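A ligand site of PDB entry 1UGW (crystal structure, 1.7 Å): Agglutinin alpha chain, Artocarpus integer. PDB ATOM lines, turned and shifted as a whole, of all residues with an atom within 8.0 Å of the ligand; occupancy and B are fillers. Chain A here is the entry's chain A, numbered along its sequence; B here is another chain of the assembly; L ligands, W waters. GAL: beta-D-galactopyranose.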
ATOM      1  N   GLY A   1       4.256  30.108 -21.560  1.00  0.00           N
ATOM      2  CA  GLY A   1       4.814  31.185 -22.418  1.00  0.00           C
ATOM      3  C   GLY A   1       4.457  32.563 -21.896  1.00  0.00           C
ATOM      4  O   GLY A   1       3.806  32.696 -20.855  1.00  0.00           O
ATOM      5  N   LYS A   2       4.873  33.594 -22.627  1.00  0.00           N
ATOM      6  CA  LYS A   2       4.591  34.973 -22.235  1.00  0.00           C
ATOM      7  C   LYS A   2       3.288  35.423 -22.884  1.00  0.00           C
ATOM      8  O   LYS A   2       3.186  35.453 -24.106  1.00  0.00           O
ATOM      9  CB  LYS A   2       5.725  35.889 -22.665  1.00  0.00           C
ATOM     10  CG  LYS A   2       5.523  37.340 -22.268  1.00  0.00           C
ATOM     11  CD  LYS A   2       6.652  38.224 -22.791  1.00  0.00           C
ATOM     12  CE  LYS A   2       6.444  39.676 -22.382  1.00  0.00           C
ATOM     13  NZ  LYS A   2       7.536  40.556 -22.905  1.00  0.00           N
ATOM     14  N   ALA A  24       6.247  24.344 -35.187  1.00  0.00           N
ATOM     15  CA  ALA A  24       5.037  25.151 -35.039  1.00  0.00           C
ATOM     16  C   ALA A  24       5.256  26.633 -35.344  1.00  0.00           C
ATOM     17  O   ALA A  24       6.318  27.030 -35.823  1.00  0.00           O
ATOM     18  CB  ALA A  24       4.486  24.992 -33.619  1.00  0.00           C
ATOM     19  N   ILE A  25       4.238  27.442 -35.049  1.00  0.00           N
ATOM     20  CA  ILE A  25       4.303  28.887 -35.263  1.00  0.00           C
ATOM     21  C   ILE A  25       5.191  29.508 -34.187  1.00  0.00           C
ATOM     22  O   ILE A  25       5.161  29.079 -33.029  1.00  0.00           O
ATOM     23  CB  ILE A  25       2.890  29.529 -35.150  1.00  0.00           C
ATOM     24  CG1 ILE A  25       1.945  28.932 -36.192  1.00  0.00           C
ATOM     25  CG2 ILE A  25       2.992  31.050 -35.301  1.00  0.00           C
ATOM     26  CD1 ILE A  25       2.352  29.174 -37.621  1.00  0.00           C
ATOM     27  N   SER A  46       9.240  34.460 -30.142  1.00  0.00           N
ATOM     28  CA  SER A  46       9.483  33.155 -29.533  1.00  0.00           C
ATOM     29  C   SER A  46      10.740  33.273 -28.668  1.00  0.00           C
ATOM     30  O   SER A  46      11.563  34.161 -28.892  1.00  0.00           O
ATOM     31  CB  SER A  46       9.716  32.113 -30.620  1.00  0.00           C
ATOM     32  OG  SER A  46      10.407  30.981 -30.102  1.00  0.00           O
ATOM     33  N   PHE A  47      10.892  32.375 -27.699  1.00  0.00           N
ATOM     34  CA  PHE A  47      12.069  32.378 -26.850  1.00  0.00           C
ATOM     35  C   PHE A  47      13.291  31.868 -27.614  1.00  0.00           C
ATOM     36  O   PHE A  47      14.418  32.101 -27.207  1.00  0.00           O
ATOM     37  CB  PHE A  47      11.869  31.486 -25.610  1.00  0.00           C
ATOM     38  CG  PHE A  47      10.777  31.959 -24.691  1.00  0.00           C
ATOM     39  CD1 PHE A  47      10.360  33.289 -24.680  1.00  0.00           C
ATOM     40  CD2 PHE A  47      10.189  31.071 -23.795  1.00  0.00           C
ATOM     41  CE1 PHE A  47       9.376  33.726 -23.803  1.00  0.00           C
ATOM     42  CE2 PHE A  47       9.203  31.496 -22.910  1.00  0.00           C
ATOM     43  CZ  PHE A  47       8.800  32.822 -22.915  1.00  0.00           C
ATOM     44  N   ILE A  48      13.045  31.162 -28.715  1.00  0.00           N
ATOM     45  CA  ILE A  48      14.125  30.616 -29.531  1.00  0.00           C
ATOM     46  C   ILE A  48      14.125  31.179 -30.957  1.00  0.00           C
ATOM     47  O   ILE A  48      13.268  31.982 -31.305  1.00  0.00           O
ATOM     48  CB  ILE A  48      14.059  29.069 -29.601  1.00  0.00           C
ATOM     49  CG1 ILE A  48      12.686  28.622 -30.118  1.00  0.00           C
ATOM     50  CG2 ILE A  48      14.324  28.473 -28.232  1.00  0.00           C
ATOM     51  CD1 ILE A  48      12.547  27.131 -30.282  1.00  0.00           C
ATOM     52  N   VAL A  75       4.157  19.517 -29.334  1.00  0.00           N
ATOM     53  CA  VAL A  75       5.511  19.740 -29.828  1.00  0.00           C
ATOM     54  C   VAL A  75       6.177  19.457 -28.499  1.00  0.00           C
ATOM     55  O   VAL A  75       6.031  20.224 -27.533  1.00  0.00           O
ATOM     56  CB  VAL A  75       5.770  21.176 -30.297  1.00  0.00           C
ATOM     57  CG1 VAL A  75       7.253  21.349 -30.596  1.00  0.00           C
ATOM     58  CG2 VAL A  75       4.963  21.454 -31.563  1.00  0.00           C
ATOM     59  N   SER A  76       6.907  18.346 -28.441  1.00  0.00           N
ATOM     60  CA  SER A  76       7.502  17.893 -27.188  1.00  0.00           C
ATOM     61  C   SER A  76       6.271  17.677 -26.299  1.00  0.00           C
ATOM     62  O   SER A  76       5.266  17.134 -26.759  1.00  0.00           O
ATOM     63  CB  SER A  76       8.467  18.924 -26.610  1.00  0.00           C
ATOM     64  OG  SER A  76       9.720  18.848 -27.281  1.00  0.00           O
ATOM     65  N   GLY A  77       6.300  18.114 -25.041  1.00  0.00           N
ATOM     66  CA  GLY A  77       5.140  17.890 -24.196  1.00  0.00           C
ATOM     67  C   GLY A  77       4.053  18.950 -24.245  1.00  0.00           C
ATOM     68  O   GLY A  77       2.948  18.740 -23.759  1.00  0.00           O
ATOM     69  N   TYR A  78       4.370  20.086 -24.876  1.00  0.00           N
ATOM     70  CA  TYR A  78       3.454  21.222 -24.957  1.00  0.00           C
ATOM     71  C   TYR A  78       2.415  21.227 -26.073  1.00  0.00           C
ATOM     72  O   TYR A  78       2.711  20.853 -27.208  1.00  0.00           O
ATOM     73  CB  TYR A  78       4.280  22.496 -25.049  1.00  0.00           C
ATOM     74  CG  TYR A  78       5.240  22.682 -23.903  1.00  0.00           C
ATOM     75  CD1 TYR A  78       4.773  23.081 -22.644  1.00  0.00           C
ATOM     76  CD2 TYR A  78       6.607  22.460 -24.065  1.00  0.00           C
ATOM     77  CE1 TYR A  78       5.643  23.242 -21.575  1.00  0.00           C
ATOM     78  CE2 TYR A  78       7.489  22.614 -22.990  1.00  0.00           C
ATOM     79  CZ  TYR A  78       7.000  23.015 -21.756  1.00  0.00           C
ATOM     80  OH  TYR A  78       7.862  23.179 -20.683  1.00  0.00           O
ATOM     81  N   VAL A  79       1.197  21.639 -25.755  1.00  0.00           N
ATOM     82  CA  VAL A  79       0.157  21.756 -26.766  1.00  0.00           C
ATOM     83  C   VAL A  79       0.319  23.159 -27.322  1.00  0.00           C
ATOM     84  O   VAL A  79       0.318  24.136 -26.561  1.00  0.00           O
ATOM     85  CB  VAL A  79      -1.265  21.598 -26.169  1.00  0.00           C
ATOM     86  CG1 VAL A  79      -2.297  21.897 -27.242  1.00  0.00           C
ATOM     87  CG2 VAL A  79      -1.460  20.192 -25.636  1.00  0.00           C
ATOM     88  N   VAL A  80       0.488  23.280 -28.635  1.00  0.00           N
ATOM     89  CA  VAL A  80       0.666  24.593 -29.252  1.00  0.00           C
ATOM     90  C   VAL A  80      -0.070  24.687 -30.576  1.00  0.00           C
ATOM     91  O   VAL A  80      -0.694  23.722 -31.025  1.00  0.00           O
ATOM     92  CB  VAL A  80       2.163  24.879 -29.525  1.00  0.00           C
ATOM     93  CG1 VAL A  80       2.959  24.838 -28.227  1.00  0.00           C
ATOM     94  CG2 VAL A  80       2.711  23.853 -30.520  1.00  0.00           C
ATOM     95  N   VAL A  81      -0.017  25.871 -31.188  1.00  0.00           N
ATOM     96  CA  VAL A  81      -0.633  26.081 -32.486  1.00  0.00           C
ATOM     97  C   VAL A  81       0.442  25.717 -33.502  1.00  0.00           C
ATOM     98  O   VAL A  81       1.418  26.436 -33.687  1.00  0.00           O
ATOM     99  CB  VAL A  81      -1.047  27.556 -32.676  1.00  0.00           C
ATOM    100  CG1 VAL A  81      -1.623  27.758 -34.064  1.00  0.00           C
ATOM    101  CG2 VAL A  81      -2.074  27.937 -31.617  1.00  0.00           C
ATOM    102  N   SER A 119      -0.446  33.719 -26.263  1.00  0.00           N
ATOM    103  CA  SER A 119       0.748  33.452 -25.480  1.00  0.00           C
ATOM    104  C   SER A 119       1.788  32.765 -26.353  1.00  0.00           C
ATOM    105  O   SER A 119       1.458  31.935 -27.191  1.00  0.00           O
ATOM    106  CB  SER A 119       0.402  32.548 -24.296  1.00  0.00           C
ATOM    107  OG  SER A 119       1.569  32.158 -23.589  1.00  0.00           O
ATOM    108  N   ILE A 120       3.048  33.137 -26.166  1.00  0.00           N
ATOM    109  CA  ILE A 120       4.134  32.547 -26.920  1.00  0.00           C
ATOM    110  C   ILE A 120       5.315  32.239 -26.013  1.00  0.00           C
ATOM    111  O   ILE A 120       5.764  33.099 -25.258  1.00  0.00           O
ATOM    112  CB  ILE A 120       4.630  33.494 -28.041  1.00  0.00           C
ATOM    113  CG1 ILE A 120       3.481  33.858 -28.986  1.00  0.00           C
ATOM    114  CG2 ILE A 120       5.761  32.819 -28.821  1.00  0.00           C
ATOM    115  CD1 ILE A 120       3.897  34.747 -30.153  1.00  0.00           C
ATOM    116  N   GLY A 121       5.781  31.004 -26.090  1.00  0.00           N
ATOM    117  CA  GLY A 121       6.947  30.564 -25.331  1.00  0.00           C
ATOM    118  C   GLY A 121       7.925  30.188 -26.428  1.00  0.00           C
ATOM    119  O   GLY A 121       8.410  31.060 -27.134  1.00  0.00           O
ATOM    120  N   TYR A 122       8.210  28.904 -26.580  1.00  0.00           N
ATOM    121  CA  TYR A 122       9.073  28.472 -27.667  1.00  0.00           C
ATOM    122  C   TYR A 122       8.215  28.639 -28.913  1.00  0.00           C
ATOM    123  O   TYR A 122       8.701  28.993 -29.993  1.00  0.00           O
ATOM    124  CB  TYR A 122       9.466  27.003 -27.534  1.00  0.00           C
ATOM    125  CG  TYR A 122      10.421  26.691 -26.409  1.00  0.00           C
ATOM    126  CD1 TYR A 122      11.536  27.486 -26.175  1.00  0.00           C
ATOM    127  CD2 TYR A 122      10.231  25.554 -25.613  1.00  0.00           C
ATOM    128  CE1 TYR A 122      12.448  27.164 -25.168  1.00  0.00           C
ATOM    129  CE2 TYR A 122      11.135  25.235 -24.603  1.00  0.00           C
ATOM    130  CZ  TYR A 122      12.244  26.035 -24.388  1.00  0.00           C
ATOM    131  OH  TYR A 122      13.156  25.695 -23.418  1.00  0.00           O
ATOM    132  N   TRP A 123       6.926  28.354 -28.756  1.00  0.00           N
ATOM    133  CA  TRP A 123       5.963  28.454 -29.848  1.00  0.00           C
ATOM    134  C   TRP A 123       4.675  29.130 -29.387  1.00  0.00           C
ATOM    135  O   TRP A 123       4.484  29.402 -28.202  1.00  0.00           O
ATOM    136  CB  TRP A 123       5.645  27.049 -30.387  1.00  0.00           C
ATOM    137  CG  TRP A 123       6.887  26.272 -30.742  1.00  0.00           C
ATOM    138  CD1 TRP A 123       7.697  26.479 -31.818  1.00  0.00           C
ATOM    139  CD2 TRP A 123       7.530  25.265 -29.940  1.00  0.00           C
ATOM    140  NE1 TRP A 123       8.815  25.669 -31.734  1.00  0.00           N
ATOM    141  CE2 TRP A 123       8.728  24.912 -30.591  1.00  0.00           C
ATOM    142  CE3 TRP A 123       7.205  24.628 -28.735  1.00  0.00           C
ATOM    143  CZ2 TRP A 123       9.611  23.954 -30.075  1.00  0.00           C
ATOM    144  CZ3 TRP A 123       8.080  23.675 -28.216  1.00  0.00           C
ATOM    145  CH2 TRP A 123       9.269  23.350 -28.890  1.00  0.00           C
ATOM    146  N   LEU A 124       3.805  29.427 -30.348  1.00  0.00           N
ATOM    147  CA  LEU A 124       2.522  30.050 -30.043  1.00  0.00           C
ATOM    148  C   LEU A 124       1.693  29.025 -29.271  1.00  0.00           C
ATOM    149  O   LEU A 124       1.248  28.021 -29.839  1.00  0.00           O
ATOM    150  CB  LEU A 124       1.821  30.427 -31.358  1.00  0.00           C
ATOM    151  CG  LEU A 124       0.447  31.096 -31.260  1.00  0.00           C
ATOM    152  CD1 LEU A 124       0.541  32.405 -30.484  1.00  0.00           C
ATOM    153  CD2 LEU A 124      -0.082  31.345 -32.672  1.00  0.00           C
ATOM    154  N   ASP A 125       1.497  29.267 -27.984  1.00  0.00           N
ATOM    155  CA  ASP A 125       0.743  28.373 -27.115  1.00  0.00           C
ATOM    156  C   ASP A 125      -0.751  28.331 -27.425  1.00  0.00           C
ATOM    157  O   ASP A 125      -1.352  27.258 -27.511  1.00  0.00           O
ATOM    158  CB  ASP A 125       0.926  28.779 -25.653  1.00  0.00           C
ATOM    159  CG  ASP A 125       2.396  28.787 -25.226  1.00  0.00           C
ATOM    160  OD1 ASP A 125       3.062  27.744 -25.389  1.00  0.00           O
ATOM    161  OD2 ASP A 125       2.862  29.836 -24.739  1.00  0.00           O
ATOM    162  N   TYR A 126      -1.345  29.507 -27.562  1.00  0.00           N
ATOM    163  CA  TYR A 126      -2.761  29.625 -27.854  1.00  0.00           C
ATOM    164  C   TYR A 126      -3.026  31.055 -28.284  1.00  0.00           C
ATOM    165  O   TYR A 126      -2.175  31.930 -28.121  1.00  0.00           O
ATOM    166  CB  TYR A 126      -3.593  29.309 -26.605  1.00  0.00           C
ATOM    167  CG  TYR A 126      -3.281  30.172 -25.398  1.00  0.00           C
ATOM    168  CD1 TYR A 126      -3.786  31.467 -25.283  1.00  0.00           C
ATOM    169  CD2 TYR A 126      -2.487  29.680 -24.357  1.00  0.00           C
ATOM    170  CE1 TYR A 126      -3.513  32.261 -24.179  1.00  0.00           C
ATOM    171  CE2 TYR A 126      -2.208  30.469 -23.234  1.00  0.00           C
ATOM    172  CZ  TYR A 126      -2.722  31.749 -23.153  1.00  0.00           C
ATOM    173  OH  TYR A 126      -2.457  32.525 -22.051  1.00  0.00           O
ATOM    174  N   ALA B  17      -3.254  25.529 -26.272  1.00  0.00           N
ATOM    175  CA  ALA B  17      -3.154  25.014 -24.907  1.00  0.00           C
ATOM    176  C   ALA B  17      -4.289  25.548 -24.045  1.00  0.00           C
ATOM    177  O   ALA B  17      -4.727  26.686 -24.218  1.00  0.00           O
ATOM    178  CB  ALA B  17      -1.806  25.408 -24.310  1.00  0.00           C
HETATM  179  C1  GAL L   1       8.369  27.048 -23.083  1.00  0.00           C
HETATM  180  C2  GAL L   1       7.535  27.611 -21.895  1.00  0.00           C
HETATM  181  C3  GAL L   1       6.200  26.858 -21.750  1.00  0.00           C
HETATM  182  C4  GAL L   1       5.451  26.850 -23.107  1.00  0.00           C
HETATM  183  C5  GAL L   1       6.388  26.242 -24.144  1.00  0.00           C
HETATM  184  C6  GAL L   1       5.758  26.088 -25.511  1.00  0.00           C
HETATM  185  O1  GAL L   1       9.470  27.857 -23.315  1.00  0.00           O
HETATM  186  O2  GAL L   1       8.282  27.482 -20.702  1.00  0.00           O
HETATM  187  O3  GAL L   1       5.420  27.543 -20.784  1.00  0.00           O
HETATM  188  O4  GAL L   1       5.121  28.181 -23.478  1.00  0.00           O
HETATM  189  O5  GAL L   1       7.579  27.052 -24.274  1.00  0.00           O
HETATM  190  O6  GAL L   1       5.690  27.326 -26.191  1.00  0.00           O
HETATM  191  O   HOH W   1       2.912  27.079 -20.420  1.00  0.00           O
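CD2 of Phe 47 touches O1 of the ligand (3.3 Å). Tyr 78 touches the ligand (CE1 to C3, 3.7 Å). Gly 121 touches the ligand. Hydrophobic or aromatic side chains that line the ligand: Phe 47, Tyr 78, Tyr 122 and Trp 123. The nearest printed residue that does not touch the ligand is Val 80 (4.1 Å).
OD1 of Asp 125 lies within hydrogen-bond range of O6 of the ligand (2.8 Å). An oxygen (O4) of the ligand is in hydrogen-bond range of the backbone NH of Gly 1, 2.9 Å away. N of Tyr 122 sits at hydrogen-bond distance from O6 of the ligand, at 3.0 Å. O6 of the ligand is in hydrogen-bond range of N of Trp 123 (3.0 Å). The backbone carbonyl oxygen (O) of Trp 123 is in hydrogen-bond range of an oxygen (O6) of the ligand (3.1 Å).
The backbone NH (N) of Gly 1 sits close to the side-chain carboxylate (OD2) of Asp 125, at 3.5 Å. The side-chain carboxylate (OD2) of Asp 125 sits at hydrogen-bond distance from the backbone NH (N) of Gly 121, at 3.4 Å. The backbone carbonyl oxygen (O) of Ser 119 sits at hydrogen-bond distance from the backbone NH (N) of Asp 125, 2.8 Å away. O of Asp 125 is in hydrogen-bond range of N of Ala 17 of chain B (2.9 Å). The side-chain hydroxyl of Ser 46 lies within hydrogen-bond range of the backbone carbonyl oxygen of Tyr 122, 2.6 Å away. The backbone NH (N) of Phe 47 sits at hydrogen-bond distance from the backbone carbonyl oxygen (O) of Gly 121.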
